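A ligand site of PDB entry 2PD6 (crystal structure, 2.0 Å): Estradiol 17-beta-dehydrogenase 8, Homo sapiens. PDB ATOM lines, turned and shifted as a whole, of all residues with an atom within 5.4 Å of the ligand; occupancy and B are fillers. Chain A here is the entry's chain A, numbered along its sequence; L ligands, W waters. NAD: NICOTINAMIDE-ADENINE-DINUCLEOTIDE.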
ATOM      1  N   THR A  13       7.156  30.747 -12.760  1.00  0.00           N
ATOM      2  CA  THR A  13       6.917  30.520 -11.321  1.00  0.00           C
ATOM      3  C   THR A  13       7.546  29.217 -10.914  1.00  0.00           C
ATOM      4  O   THR A  13       7.771  28.333 -11.733  1.00  0.00           O
ATOM      5  CB  THR A  13       5.407  30.537 -10.938  1.00  0.00           C
ATOM      6  OG1 THR A  13       4.800  29.345 -11.438  1.00  0.00           O
ATOM      7  CG2 THR A  13       4.682  31.789 -11.487  1.00  0.00           C
ATOM      8  N   GLY A  14       7.921  29.109  -9.645  1.00  0.00           N
ATOM      9  CA  GLY A  14       8.780  27.984  -9.195  1.00  0.00           C
ATOM     10  C   GLY A  14      10.132  27.963  -9.894  1.00  0.00           C
ATOM     11  O   GLY A  14      10.739  26.881 -10.066  1.00  0.00           O
ATOM     12  N   ALA A  15      10.617  29.147 -10.265  1.00  0.00           N
ATOM     13  CA  ALA A  15      11.875  29.327 -11.001  1.00  0.00           C
ATOM     14  C   ALA A  15      13.126  29.075 -10.187  1.00  0.00           C
ATOM     15  O   ALA A  15      14.261  29.040 -10.731  1.00  0.00           O
ATOM     16  CB  ALA A  15      11.927  30.749 -11.627  1.00  0.00           C
ATOM     17  N   GLY A  16      12.948  28.893  -8.885  1.00  0.00           N
ATOM     18  CA  GLY A  16      14.040  28.732  -7.966  1.00  0.00           C
ATOM     19  C   GLY A  16      14.657  27.343  -7.927  1.00  0.00           C
ATOM     20  O   GLY A  16      15.754  27.185  -7.401  1.00  0.00           O
ATOM     21  N   SER A  17      13.998  26.328  -8.500  1.00  0.00           N
ATOM     22  CA  SER A  17      14.522  24.955  -8.394  1.00  0.00           C
ATOM     23  C   SER A  17      14.105  24.097  -9.574  1.00  0.00           C
ATOM     24  O   SER A  17      13.187  24.449 -10.265  1.00  0.00           O
ATOM     25  CB  SER A  17      13.985  24.312  -7.106  1.00  0.00           C
ATOM     26  OG  SER A  17      14.580  23.037  -6.912  1.00  0.00           O
ATOM     27  N   GLY A  18      14.755  22.964  -9.756  1.00  0.00           N
ATOM     28  CA  GLY A  18      14.294  21.895 -10.652  1.00  0.00           C
ATOM     29  C   GLY A  18      13.849  22.337 -12.033  1.00  0.00           C
ATOM     30  O   GLY A  18      14.639  22.867 -12.821  1.00  0.00           O
ATOM     31  N   ILE A  19      12.611  22.019 -12.354  1.00  0.00           N
ATOM     32  CA  ILE A  19      12.069  22.275 -13.691  1.00  0.00           C
ATOM     33  C   ILE A  19      11.960  23.769 -13.948  1.00  0.00           C
ATOM     34  O   ILE A  19      12.308  24.254 -15.011  1.00  0.00           O
ATOM     35  CB  ILE A  19      10.687  21.580 -13.902  1.00  0.00           C
ATOM     36  CG1 ILE A  19      10.869  20.039 -13.902  1.00  0.00           C
ATOM     37  CG2 ILE A  19      10.040  22.044 -15.191  1.00  0.00           C
ATOM     38  CD1 ILE A  19       9.514  19.274 -13.898  1.00  0.00           C
ATOM     39  N   GLY A  20      11.515  24.505 -12.978  1.00  0.00           N
ATOM     40  CA  GLY A  20      11.433  25.957 -13.124  1.00  0.00           C
ATOM     41  C   GLY A  20      12.764  26.591 -13.481  1.00  0.00           C
ATOM     42  O   GLY A  20      12.831  27.474 -14.335  1.00  0.00           O
ATOM     43  N   CYS A  37      10.219  33.907 -10.792  1.00  0.00           N
ATOM     44  CA  CYS A  37       9.415  34.035  -9.564  1.00  0.00           C
ATOM     45  C   CYS A  37       9.490  32.748  -8.729  1.00  0.00           C
ATOM     46  O   CYS A  37       9.349  31.634  -9.267  1.00  0.00           O
ATOM     47  CB  CYS A  37       7.964  34.283  -9.959  1.00  0.00           C
ATOM     48  SG  CYS A  37       6.805  34.169  -8.560  1.00  0.00           S
ATOM     49  N   ASP A  38       9.643  32.907  -7.424  1.00  0.00           N
ATOM     50  CA  ASP A  38       9.599  31.748  -6.513  1.00  0.00           C
ATOM     51  C   ASP A  38       9.072  32.204  -5.151  1.00  0.00           C
ATOM     52  O   ASP A  38       9.139  33.388  -4.785  1.00  0.00           O
ATOM     53  CB  ASP A  38      11.011  31.114  -6.369  1.00  0.00           C
ATOM     54  CG  ASP A  38      10.951  29.649  -5.931  1.00  0.00           C
ATOM     55  OD1 ASP A  38      10.899  29.437  -4.724  1.00  0.00           O
ATOM     56  OD2 ASP A  38      10.872  28.714  -6.793  1.00  0.00           O
ATOM     57  N   LEU A  39       8.529  31.279  -4.389  1.00  0.00           N
ATOM     58  CA  LEU A  39       8.162  31.550  -3.013  1.00  0.00           C
ATOM     59  C   LEU A  39       9.403  32.001  -2.229  1.00  0.00           C
ATOM     60  O   LEU A  39       9.317  32.806  -1.290  1.00  0.00           O
ATOM     61  CB  LEU A  39       7.619  30.251  -2.403  1.00  0.00           C
ATOM     62  CG  LEU A  39       7.245  30.229  -0.939  1.00  0.00           C
ATOM     63  CD1 LEU A  39       6.047  31.130  -0.716  1.00  0.00           C
ATOM     64  CD2 LEU A  39       6.947  28.795  -0.471  1.00  0.00           C
ATOM     65  N   ASP A  40      10.557  31.443  -2.605  1.00  0.00           N
ATOM     66  CA  ASP A  40      11.829  31.691  -1.915  1.00  0.00           C
ATOM     67  C   ASP A  40      12.597  32.658  -2.781  1.00  0.00           C
ATOM     68  O   ASP A  40      13.057  32.314  -3.858  1.00  0.00           O
ATOM     69  CB  ASP A  40      12.554  30.360  -1.758  1.00  0.00           C
ATOM     70  CG  ASP A  40      13.951  30.501  -1.263  1.00  0.00           C
ATOM     71  OD1 ASP A  40      14.404  31.632  -0.940  1.00  0.00           O
ATOM     72  OD2 ASP A  40      14.627  29.459  -1.172  1.00  0.00           O
ATOM     73  N   ALA A  43      16.083  31.783  -3.950  1.00  0.00           N
ATOM     74  CA  ALA A  43      16.158  30.745  -4.985  1.00  0.00           C
ATOM     75  C   ALA A  43      15.943  31.359  -6.379  1.00  0.00           C
ATOM     76  O   ALA A  43      16.619  31.009  -7.347  1.00  0.00           O
ATOM     77  CB  ALA A  43      15.115  29.631  -4.728  1.00  0.00           C
ATOM     78  N   ALA A  70       6.924  35.630  -4.715  1.00  0.00           N
ATOM     79  CA  ALA A  70       5.471  35.516  -4.618  1.00  0.00           C
ATOM     80  C   ALA A  70       5.018  34.142  -4.124  1.00  0.00           C
ATOM     81  O   ALA A  70       5.613  33.129  -4.473  1.00  0.00           O
ATOM     82  CB  ALA A  70       4.826  35.826  -5.986  1.00  0.00           C
ATOM     83  N   ASP A  71       3.978  34.118  -3.299  1.00  0.00           N
ATOM     84  CA  ASP A  71       3.249  32.868  -3.035  1.00  0.00           C
ATOM     85  C   ASP A  71       2.064  32.842  -3.980  1.00  0.00           C
ATOM     86  O   ASP A  71       1.092  33.535  -3.743  1.00  0.00           O
ATOM     87  CB  ASP A  71       2.780  32.818  -1.573  1.00  0.00           C
ATOM     88  CG  ASP A  71       2.156  31.472  -1.200  1.00  0.00           C
ATOM     89  OD1 ASP A  71       1.840  30.654  -2.120  1.00  0.00           O
ATOM     90  OD2 ASP A  71       1.998  31.235   0.033  1.00  0.00           O
ATOM     91  N   VAL A  72       2.138  32.025  -5.029  1.00  0.00           N
ATOM     92  CA  VAL A  72       1.125  32.020  -6.108  1.00  0.00           C
ATOM     93  C   VAL A  72      -0.238  31.461  -5.681  1.00  0.00           C
ATOM     94  O   VAL A  72      -1.219  31.607  -6.405  1.00  0.00           O
ATOM     95  CB  VAL A  72       1.572  31.205  -7.359  1.00  0.00           C
ATOM     96  CG1 VAL A  72       2.859  31.785  -7.971  1.00  0.00           C
ATOM     97  CG2 VAL A  72       1.755  29.707  -7.022  1.00  0.00           C
ATOM     98  N   SER A  73      -0.301  30.789  -4.534  1.00  0.00           N
ATOM     99  CA  SER A  73      -1.576  30.353  -3.998  1.00  0.00           C
ATOM    100  C   SER A  73      -2.411  31.533  -3.433  1.00  0.00           C
ATOM    101  O   SER A  73      -3.602  31.408  -3.247  1.00  0.00           O
ATOM    102  CB  SER A  73      -1.366  29.273  -2.947  1.00  0.00           C
ATOM    103  OG  SER A  73      -0.832  29.802  -1.754  1.00  0.00           O
ATOM    104  N   SER A  98       3.905  28.022 -15.388  1.00  0.00           N
ATOM    105  CA  SER A  98       3.604  27.749 -14.004  1.00  0.00           C
ATOM    106  C   SER A  98       4.271  26.445 -13.636  1.00  0.00           C
ATOM    107  O   SER A  98       3.808  25.384 -14.024  1.00  0.00           O
ATOM    108  CB  SER A  98       2.079  27.673 -13.809  1.00  0.00           C
ATOM    109  OG  SER A  98       1.522  28.984 -13.605  1.00  0.00           O
ATOM    110  N   CYS A  99       5.389  26.531 -12.904  1.00  0.00           N
ATOM    111  CA  CYS A  99       6.097  25.337 -12.410  1.00  0.00           C
ATOM    112  C   CYS A  99       6.098  25.222 -10.918  1.00  0.00           C
ATOM    113  O   CYS A  99       6.695  24.307 -10.409  1.00  0.00           O
ATOM    114  CB  CYS A  99       7.584  25.286 -12.860  1.00  0.00           C
ATOM    115  SG  CYS A  99       7.958  25.688 -14.575  1.00  0.00           S
ATOM    116  N   ALA A 100       5.466  26.161 -10.215  1.00  0.00           N
ATOM    117  CA  ALA A 100       5.389  26.133  -8.765  1.00  0.00           C
ATOM    118  C   ALA A 100       4.468  24.991  -8.423  1.00  0.00           C
ATOM    119  O   ALA A 100       3.332  24.947  -8.922  1.00  0.00           O
ATOM    120  CB  ALA A 100       4.803  27.407  -8.233  1.00  0.00           C
ATOM    121  N   GLY A 101       4.943  24.090  -7.567  1.00  0.00           N
ATOM    122  CA  GLY A 101       4.219  22.880  -7.338  1.00  0.00           C
ATOM    123  C   GLY A 101       4.827  22.180  -6.167  1.00  0.00           C
ATOM    124  O   GLY A 101       6.041  22.394  -5.844  1.00  0.00           O
ATOM    125  N   ILE A 102       4.004  21.389  -5.486  1.00  0.00           N
ATOM    126  CA  ILE A 102       4.475  20.608  -4.347  1.00  0.00           C
ATOM    127  C   ILE A 102       3.756  19.268  -4.213  1.00  0.00           C
ATOM    128  O   ILE A 102       2.723  19.038  -4.843  1.00  0.00           O
ATOM    129  CB  ILE A 102       4.270  21.352  -3.016  1.00  0.00           C
ATOM    130  CG1 ILE A 102       2.785  21.659  -2.785  1.00  0.00           C
ATOM    131  CG2 ILE A 102       5.063  22.645  -2.948  1.00  0.00           C
ATOM    132  CD1 ILE A 102       2.442  21.802  -1.321  1.00  0.00           C
ATOM    133  N   VAL A 122      -1.546  25.279  -3.642  1.00  0.00           N
ATOM    134  CA  VAL A 122      -0.358  25.593  -4.445  1.00  0.00           C
ATOM    135  C   VAL A 122      -0.501  25.137  -5.917  1.00  0.00           C
ATOM    136  O   VAL A 122      -0.392  25.932  -6.870  1.00  0.00           O
ATOM    137  CB  VAL A 122       0.925  25.014  -3.804  1.00  0.00           C
ATOM    138  CG1 VAL A 122       2.168  25.295  -4.719  1.00  0.00           C
ATOM    139  CG2 VAL A 122       1.127  25.575  -2.383  1.00  0.00           C
ATOM    140  N   ASN A 123      -0.814  23.861  -6.105  1.00  0.00           N
ATOM    141  CA  ASN A 123      -0.757  23.281  -7.450  1.00  0.00           C
ATOM    142  C   ASN A 123      -1.932  23.696  -8.340  1.00  0.00           C
ATOM    143  O   ASN A 123      -1.781  23.881  -9.574  1.00  0.00           O
ATOM    144  CB  ASN A 123      -0.719  21.766  -7.371  1.00  0.00           C
ATOM    145  CG  ASN A 123       0.532  21.230  -6.694  1.00  0.00           C
ATOM    146  OD1 ASN A 123       1.374  21.987  -6.226  1.00  0.00           O
ATOM    147  ND2 ASN A 123       0.643  19.908  -6.613  1.00  0.00           N
ATOM    148  N   ILE A 150       2.612  23.257 -15.934  1.00  0.00           N
ATOM    149  CA  ILE A 150       3.276  21.970 -15.706  1.00  0.00           C
ATOM    150  C   ILE A 150       2.320  21.172 -14.791  1.00  0.00           C
ATOM    151  O   ILE A 150       2.008  21.570 -13.659  1.00  0.00           O
ATOM    152  CB  ILE A 150       4.690  22.098 -15.087  1.00  0.00           C
ATOM    153  CG1 ILE A 150       5.533  23.137 -15.808  1.00  0.00           C
ATOM    154  CG2 ILE A 150       5.459  20.732 -15.150  1.00  0.00           C
ATOM    155  CD1 ILE A 150       5.685  22.873 -17.260  1.00  0.00           C
ATOM    156  N   SER A 151       1.798  20.082 -15.331  1.00  0.00           N
ATOM    157  CA  SER A 151       0.944  19.182 -14.588  1.00  0.00           C
ATOM    158  C   SER A 151       1.793  17.967 -14.260  1.00  0.00           C
ATOM    159  O   SER A 151       2.856  18.125 -13.676  1.00  0.00           O
ATOM    160  CB  SER A 151      -0.291  18.867 -15.414  1.00  0.00           C
ATOM    161  OG  SER A 151      -1.163  17.976 -14.740  1.00  0.00           O
ATOM    162  N   SER A 152       1.330  16.783 -14.617  1.00  0.00           N
ATOM    163  CA  SER A 152       2.072  15.551 -14.372  1.00  0.00           C
ATOM    164  C   SER A 152       1.300  14.395 -14.983  1.00  0.00           C
ATOM    165  O   SER A 152       0.053  14.445 -15.094  1.00  0.00           O
ATOM    166  CB  SER A 152       2.221  15.310 -12.854  1.00  0.00           C
ATOM    167  OG  SER A 152       2.619  13.967 -12.575  1.00  0.00           O
ATOM    168  N   ILE A 153       2.007  13.333 -15.359  1.00  0.00           N
ATOM    169  CA  ILE A 153       1.351  12.154 -15.901  1.00  0.00           C
ATOM    170  C   ILE A 153       0.425  11.559 -14.818  1.00  0.00           C
ATOM    171  O   ILE A 153      -0.557  10.879 -15.136  1.00  0.00           O
ATOM    172  CB  ILE A 153       2.372  11.112 -16.461  1.00  0.00           C
ATOM    173  CG1 ILE A 153       1.701  10.100 -17.387  1.00  0.00           C
ATOM    174  CG2 ILE A 153       3.061  10.350 -15.342  1.00  0.00           C
ATOM    175  CD1 ILE A 153       1.128  10.698 -18.681  1.00  0.00           C
ATOM    176  N   TYR A 165      -2.261  15.043  -4.916  1.00  0.00           N
ATOM    177  CA  TYR A 165      -1.448  15.506  -6.035  1.00  0.00           C
ATOM    178  C   TYR A 165      -2.112  15.171  -7.354  1.00  0.00           C
ATOM    179  O   TYR A 165      -2.224  16.034  -8.227  1.00  0.00           O
ATOM    180  CB  TYR A 165      -0.100  14.835  -5.975  1.00  0.00           C
ATOM    181  CG  TYR A 165       0.894  15.267  -7.000  1.00  0.00           C
ATOM    182  CD1 TYR A 165       1.561  16.471  -6.859  1.00  0.00           C
ATOM    183  CD2 TYR A 165       1.229  14.438  -8.074  1.00  0.00           C
ATOM    184  CE1 TYR A 165       2.546  16.875  -7.775  1.00  0.00           C
ATOM    185  CE2 TYR A 165       2.215  14.828  -9.017  1.00  0.00           C
ATOM    186  CZ  TYR A 165       2.868  16.048  -8.854  1.00  0.00           C
ATOM    187  OH  TYR A 165       3.868  16.484  -9.701  1.00  0.00           O
ATOM    188  N   LYS A 169      -3.381  17.900 -10.147  1.00  0.00           N
ATOM    189  CA  LYS A 169      -2.810  17.853 -11.456  1.00  0.00           C
ATOM    190  C   LYS A 169      -3.834  17.548 -12.536  1.00  0.00           C
ATOM    191  O   LYS A 169      -3.754  18.093 -13.637  1.00  0.00           O
ATOM    192  CB  LYS A 169      -1.607  16.883 -11.465  1.00  0.00           C
ATOM    193  CG  LYS A 169      -0.442  17.404 -10.585  1.00  0.00           C
ATOM    194  CD  LYS A 169       0.010  18.833 -10.939  1.00  0.00           C
ATOM    195  CE  LYS A 169       1.477  19.049 -10.497  1.00  0.00           C
ATOM    196  NZ  LYS A 169       2.048  20.378 -10.841  1.00  0.00           N
ATOM    197  N   PRO A 195       5.116  15.712 -17.314  1.00  0.00           N
ATOM    198  CA  PRO A 195       6.338  14.971 -17.177  1.00  0.00           C
ATOM    199  C   PRO A 195       6.133  13.652 -16.456  1.00  0.00           C
ATOM    200  O   PRO A 195       5.216  13.516 -15.615  1.00  0.00           O
ATOM    201  CB  PRO A 195       7.216  15.881 -16.321  1.00  0.00           C
ATOM    202  CG  PRO A 195       6.455  17.229 -16.267  1.00  0.00           C
ATOM    203  CD  PRO A 195       5.063  16.862 -16.391  1.00  0.00           C
ATOM    204  N   GLY A 196       7.023  12.702 -16.732  1.00  0.00           N
ATOM    205  CA  GLY A 196       7.112  11.457 -15.936  1.00  0.00           C
ATOM    206  C   GLY A 196       8.049  11.536 -14.737  1.00  0.00           C
ATOM    207  O   GLY A 196       7.941  12.446 -13.916  1.00  0.00           O
ATOM    208  N   PHE A 197       8.946  10.566 -14.595  1.00  0.00           N
ATOM    209  CA  PHE A 197       9.903  10.548 -13.500  1.00  0.00           C
ATOM    210  C   PHE A 197      11.088  11.418 -13.908  1.00  0.00           C
ATOM    211  O   PHE A 197      11.874  11.009 -14.749  1.00  0.00           O
ATOM    212  CB  PHE A 197      10.400   9.121 -13.230  1.00  0.00           C
ATOM    213  CG  PHE A 197       9.313   8.148 -12.837  1.00  0.00           C
ATOM    214  N   ILE A 198      11.182  12.618 -13.336  1.00  0.00           N
ATOM    215  CA  ILE A 198      12.293  13.534 -13.599  1.00  0.00           C
ATOM    216  C   ILE A 198      13.213  13.650 -12.382  1.00  0.00           C
ATOM    217  O   ILE A 198      12.744  13.918 -11.289  1.00  0.00           O
ATOM    218  CB  ILE A 198      11.805  14.957 -13.929  1.00  0.00           C
ATOM    219  CG1 ILE A 198      10.750  14.974 -15.051  1.00  0.00           C
ATOM    220  CG2 ILE A 198      12.978  15.844 -14.283  1.00  0.00           C
ATOM    221  CD1 ILE A 198      11.133  14.188 -16.323  1.00  0.00           C
ATOM    222  N   ALA A 199      14.517  13.459 -12.560  1.00  0.00           N
ATOM    223  CA  ALA A 199      15.478  13.709 -11.457  1.00  0.00           C
ATOM    224  C   ALA A 199      15.504  15.209 -11.107  1.00  0.00           C
ATOM    225  O   ALA A 199      16.020  16.024 -11.878  1.00  0.00           O
ATOM    226  CB  ALA A 199      16.849  13.240 -11.843  1.00  0.00           C
ATOM    227  N   THR A 200      14.890  15.577  -9.981  1.00  0.00           N
ATOM    228  CA  THR A 200      14.902  16.955  -9.447  1.00  0.00           C
ATOM    229  C   THR A 200      14.959  16.849  -7.919  1.00  0.00           C
ATOM    230  O   THR A 200      15.050  15.719  -7.393  1.00  0.00           O
ATOM    231  CB  THR A 200      13.663  17.833  -9.897  1.00  0.00           C
ATOM    232  OG1 THR A 200      12.501  17.483  -9.115  1.00  0.00           O
ATOM    233  CG2 THR A 200      13.342  17.695 -11.372  1.00  0.00           C
ATOM    234  N   PRO A 201      14.915  17.991  -7.193  1.00  0.00           N
ATOM    235  CA  PRO A 201      14.876  17.852  -5.723  1.00  0.00           C
ATOM    236  C   PRO A 201      13.525  17.363  -5.171  1.00  0.00           C
ATOM    237  O   PRO A 201      13.473  16.872  -4.043  1.00  0.00           O
ATOM    238  CB  PRO A 201      15.197  19.270  -5.218  1.00  0.00           C
ATOM    239  CG  PRO A 201      15.549  20.084  -6.425  1.00  0.00           C
ATOM    240  CD  PRO A 201      14.957  19.407  -7.603  1.00  0.00           C
ATOM    241  N   MET A 202      12.437  17.526  -5.945  1.00  0.00           N
ATOM    242  CA  MET A 202      11.116  17.035  -5.506  1.00  0.00           C
ATOM    243  C   MET A 202      11.139  15.529  -5.194  1.00  0.00           C
ATOM    244  O   MET A 202      11.706  14.732  -5.952  1.00  0.00           O
ATOM    245  CB  MET A 202      10.035  17.339  -6.534  1.00  0.00           C
ATOM    246  CG  MET A 202       8.615  17.164  -5.986  1.00  0.00           C
ATOM    247  SD  MET A 202       7.345  17.945  -6.990  1.00  0.00           S
ATOM    248  CE  MET A 202       7.073  16.652  -8.187  1.00  0.00           C
HETATM  249  PA  NAD L   1      11.098  21.608  -7.223  1.00  0.00           P
HETATM  250  O1A NAD L   1      10.701  21.429  -5.793  1.00  0.00           O
HETATM  251  O2A NAD L   1      12.487  21.329  -7.663  1.00  0.00           O
HETATM  252  O5B NAD L   1      10.654  23.122  -7.669  1.00  0.00           O
HETATM  253  C5B NAD L   1       9.426  23.689  -7.203  1.00  0.00           C
HETATM  254  C4B NAD L   1       9.591  25.172  -6.995  1.00  0.00           C
HETATM  255  O4B NAD L   1       8.263  25.548  -6.654  1.00  0.00           O
HETATM  256  C3B NAD L   1      10.466  25.422  -5.733  1.00  0.00           C
HETATM  257  O3B NAD L   1      11.495  26.381  -6.027  1.00  0.00           O
HETATM  258  C2B NAD L   1       9.517  26.029  -4.722  1.00  0.00           C
HETATM  259  O2B NAD L   1      10.202  27.064  -3.919  1.00  0.00           O
HETATM  260  C1B NAD L   1       8.472  26.606  -5.688  1.00  0.00           C
HETATM  261  N9A NAD L   1       7.198  26.842  -4.994  1.00  0.00           N
HETATM  262  C8A NAD L   1       6.545  26.004  -4.195  1.00  0.00           C
HETATM  263  N7A NAD L   1       5.446  26.614  -3.749  1.00  0.00           N
HETATM  264  C5A NAD L   1       5.392  27.846  -4.272  1.00  0.00           C
HETATM  265  C6A NAD L   1       4.488  28.916  -4.169  1.00  0.00           C
HETATM  266  N6A NAD L   1       3.399  28.806  -3.405  1.00  0.00           N
HETATM  267  N1A NAD L   1       4.728  30.051  -4.867  1.00  0.00           N
HETATM  268  C2A NAD L   1       5.838  30.134  -5.613  1.00  0.00           C
HETATM  269  N3A NAD L   1       6.747  29.144  -5.740  1.00  0.00           N
HETATM  270  C4A NAD L   1       6.518  27.996  -5.074  1.00  0.00           C
HETATM  271  O3  NAD L   1      10.066  20.677  -8.063  1.00  0.00           O
HETATM  272  PN  NAD L   1      10.149  20.321  -9.625  1.00  0.00           P
HETATM  273  O1N NAD L   1      10.421  18.857  -9.764  1.00  0.00           O
HETATM  274  O2N NAD L   1      11.002  21.310 -10.274  1.00  0.00           O
HETATM  275  O5D NAD L   1       8.596  20.495 -10.076  1.00  0.00           O
HETATM  276  C5D NAD L   1       8.153  21.609 -10.918  1.00  0.00           C
HETATM  277  C4D NAD L   1       6.696  21.371 -11.394  1.00  0.00           C
HETATM  278  O4D NAD L   1       6.682  20.143 -12.176  1.00  0.00           O
HETATM  279  C3D NAD L   1       5.701  21.136 -10.256  1.00  0.00           C
HETATM  280  O3D NAD L   1       4.440  21.515 -10.772  1.00  0.00           O
HETATM  281  C2D NAD L   1       5.739  19.616 -10.044  1.00  0.00           C
HETATM  282  O2D NAD L   1       4.567  19.089  -9.375  1.00  0.00           O
HETATM  283  C1D NAD L   1       5.802  19.162 -11.513  1.00  0.00           C
HETATM  284  N1N NAD L   1       6.266  17.741 -11.755  1.00  0.00           N
HETATM  285  C2N NAD L   1       7.517  17.248 -11.312  1.00  0.00           C
HETATM  286  C3N NAD L   1       7.898  15.929 -11.580  1.00  0.00           C
HETATM  287  C7N NAD L   1       9.254  15.341 -11.107  1.00  0.00           C
HETATM  288  O7N NAD L   1       9.466  13.999 -11.075  1.00  0.00           O
HETATM  289  N7N NAD L   1      10.204  16.196 -10.702  1.00  0.00           N
HETATM  290  C4N NAD L   1       7.036  15.089 -12.275  1.00  0.00           C
HETATM  291  C5N NAD L   1       5.798  15.561 -12.719  1.00  0.00           C
HETATM  292  C6N NAD L   1       5.408  16.865 -12.474  1.00  0.00           C
HETATM  293  O   HOH W   1      10.352  24.175 -10.439  1.00  0.00           O
HETATM  294  O   HOH W   2       3.278  23.575 -11.804  1.00  0.00           O
HETATM  295  O   HOH W   3       8.389  21.374  -4.241  1.00  0.00           O
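O of Ala 70 sits close to N1A of the ligand, at 3.2 Å. Gly 14 touches the ligand. Gly 16 touches the ligand. Cys 99 touches the ligand. CB of Ala 100 touches N3A of the ligand, 3.6 Å away. CA of Gly 101 touches O3D of the ligand (3.7 Å). Ile 102 touches the ligand (CG2 to C8A, 3.9 Å). Val 122 touches the ligand. Ile 150 touches the ligand (CG2 to O4D, 3.3 Å). O of Ser 151 touches C6N of the ligand (3.1 Å). Ser 152 touches the ligand (OG to C5N, 3.6 Å). Pro 195 touches the ligand. O of Gly 196 touches C4N of the ligand (3.2 Å). CD of Pro 201 touches O2A of the ligand, at 3.1 Å. Met 202 touches the ligand. Hydrophobic or aromatic side chains within 4 Å of the ligand: Ile 19, Leu 39, Val 72, Ala 100, Ile 102, Val 122, Ile 150, Tyr 165, Pro 195, Ile 198, Pro 201 and Met 202. 26 residues have an atom within 4 Å of the ligand: Gly 14, Gly 16, Ser 17, Gly 18, Ile 19, Asp 38, Leu 39, Ala 70, Asp 71, Val 72, Cys 99, Ala 100, Gly 101, Ile 102, Val 122, Ile 150, Ser 151, Ser 152, Tyr 165, Lys 169, Pro 195, Gly 196, Ile 198, Thr 200, Pro 201 and Met 202. The nearest printed residue that does not touch the ligand is Phe 197 (4.2 Å).
The side-chain carboxylate (OD1) of Asp 38 lies within hydrogen-bond range of the backbone NH (N) of Asp 40. O of Ile 150 sits at hydrogen-bond distance from NZ of Lys 169, at 3.1 Å. OG of Ser 73 lies within hydrogen-bond range of OD1 of Asp 71, at 2.8 Å. N of Leu 39 lies close to O of Ala 70, 3.5 Å away. The backbone carbonyl oxygen of Thr 13 lies within hydrogen-bond range of the backbone NH of Cys 99 (3.2 Å). O of Pro 195 sits at hydrogen-bond distance from N of Ile 153, 3.2 Å away. N of Ala 100 is in hydrogen-bond range of OG1 of Thr 13, at 3.5 Å. The side-chain amide oxygen (OD1) of Asn 123 is in hydrogen-bond range of the backbone NH (N) of Ile 102 (2.8 Å).
OD2 of Asp 38 is in hydrogen-bond range of O3B of the ligand (2.5 Å). The side-chain hydroxyl of Thr 200 is in hydrogen-bond range of an oxygen (O1N) of the ligand (2.6 Å). An oxygen (O3D) of the ligand lies within hydrogen-bond range of the side-chain amino group of Lys 169 (2.6 Å). An oxygen (O2D) of the ligand is in hydrogen-bond range of the side-chain hydroxyl of Tyr 165 (2.7 Å). An oxygen (O2N) of the ligand lies within hydrogen-bond range of the backbone NH (N) of Ile 19 (2.7 Å). OD1 of Asp 71 lies within hydrogen-bond range of N6A of the ligand, at 2.7 Å. OG of Ser 17 sits at hydrogen-bond distance from O2A of the ligand. The backbone NH (N) of Leu 39 sits at hydrogen-bond distance from a nitrogen (N3A) of the ligand (3.1 Å). The backbone NH (N) of Ile 198 lies within hydrogen-bond range of an oxygen (O7N) of the ligand. O of Ile 198 lies within hydrogen-bond range of N7N of the ligand (3.5 Å). A nitrogen (N1A) of the ligand lies within hydrogen-bond range of the backbone NH (N) of Val 72 (3.3 Å). An oxygen (O2A) of the ligand lies within hydrogen-bond range of the backbone NH of Gly 18.
Water W3 bridges O1A of the ligand (2.8 Å) and O of Gly 101 (3.0 Å). Water W1 lies within hydrogen-bond range of O of Gly 14, N of Gly 20, O of Ser 17 and O2N of the ligand.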
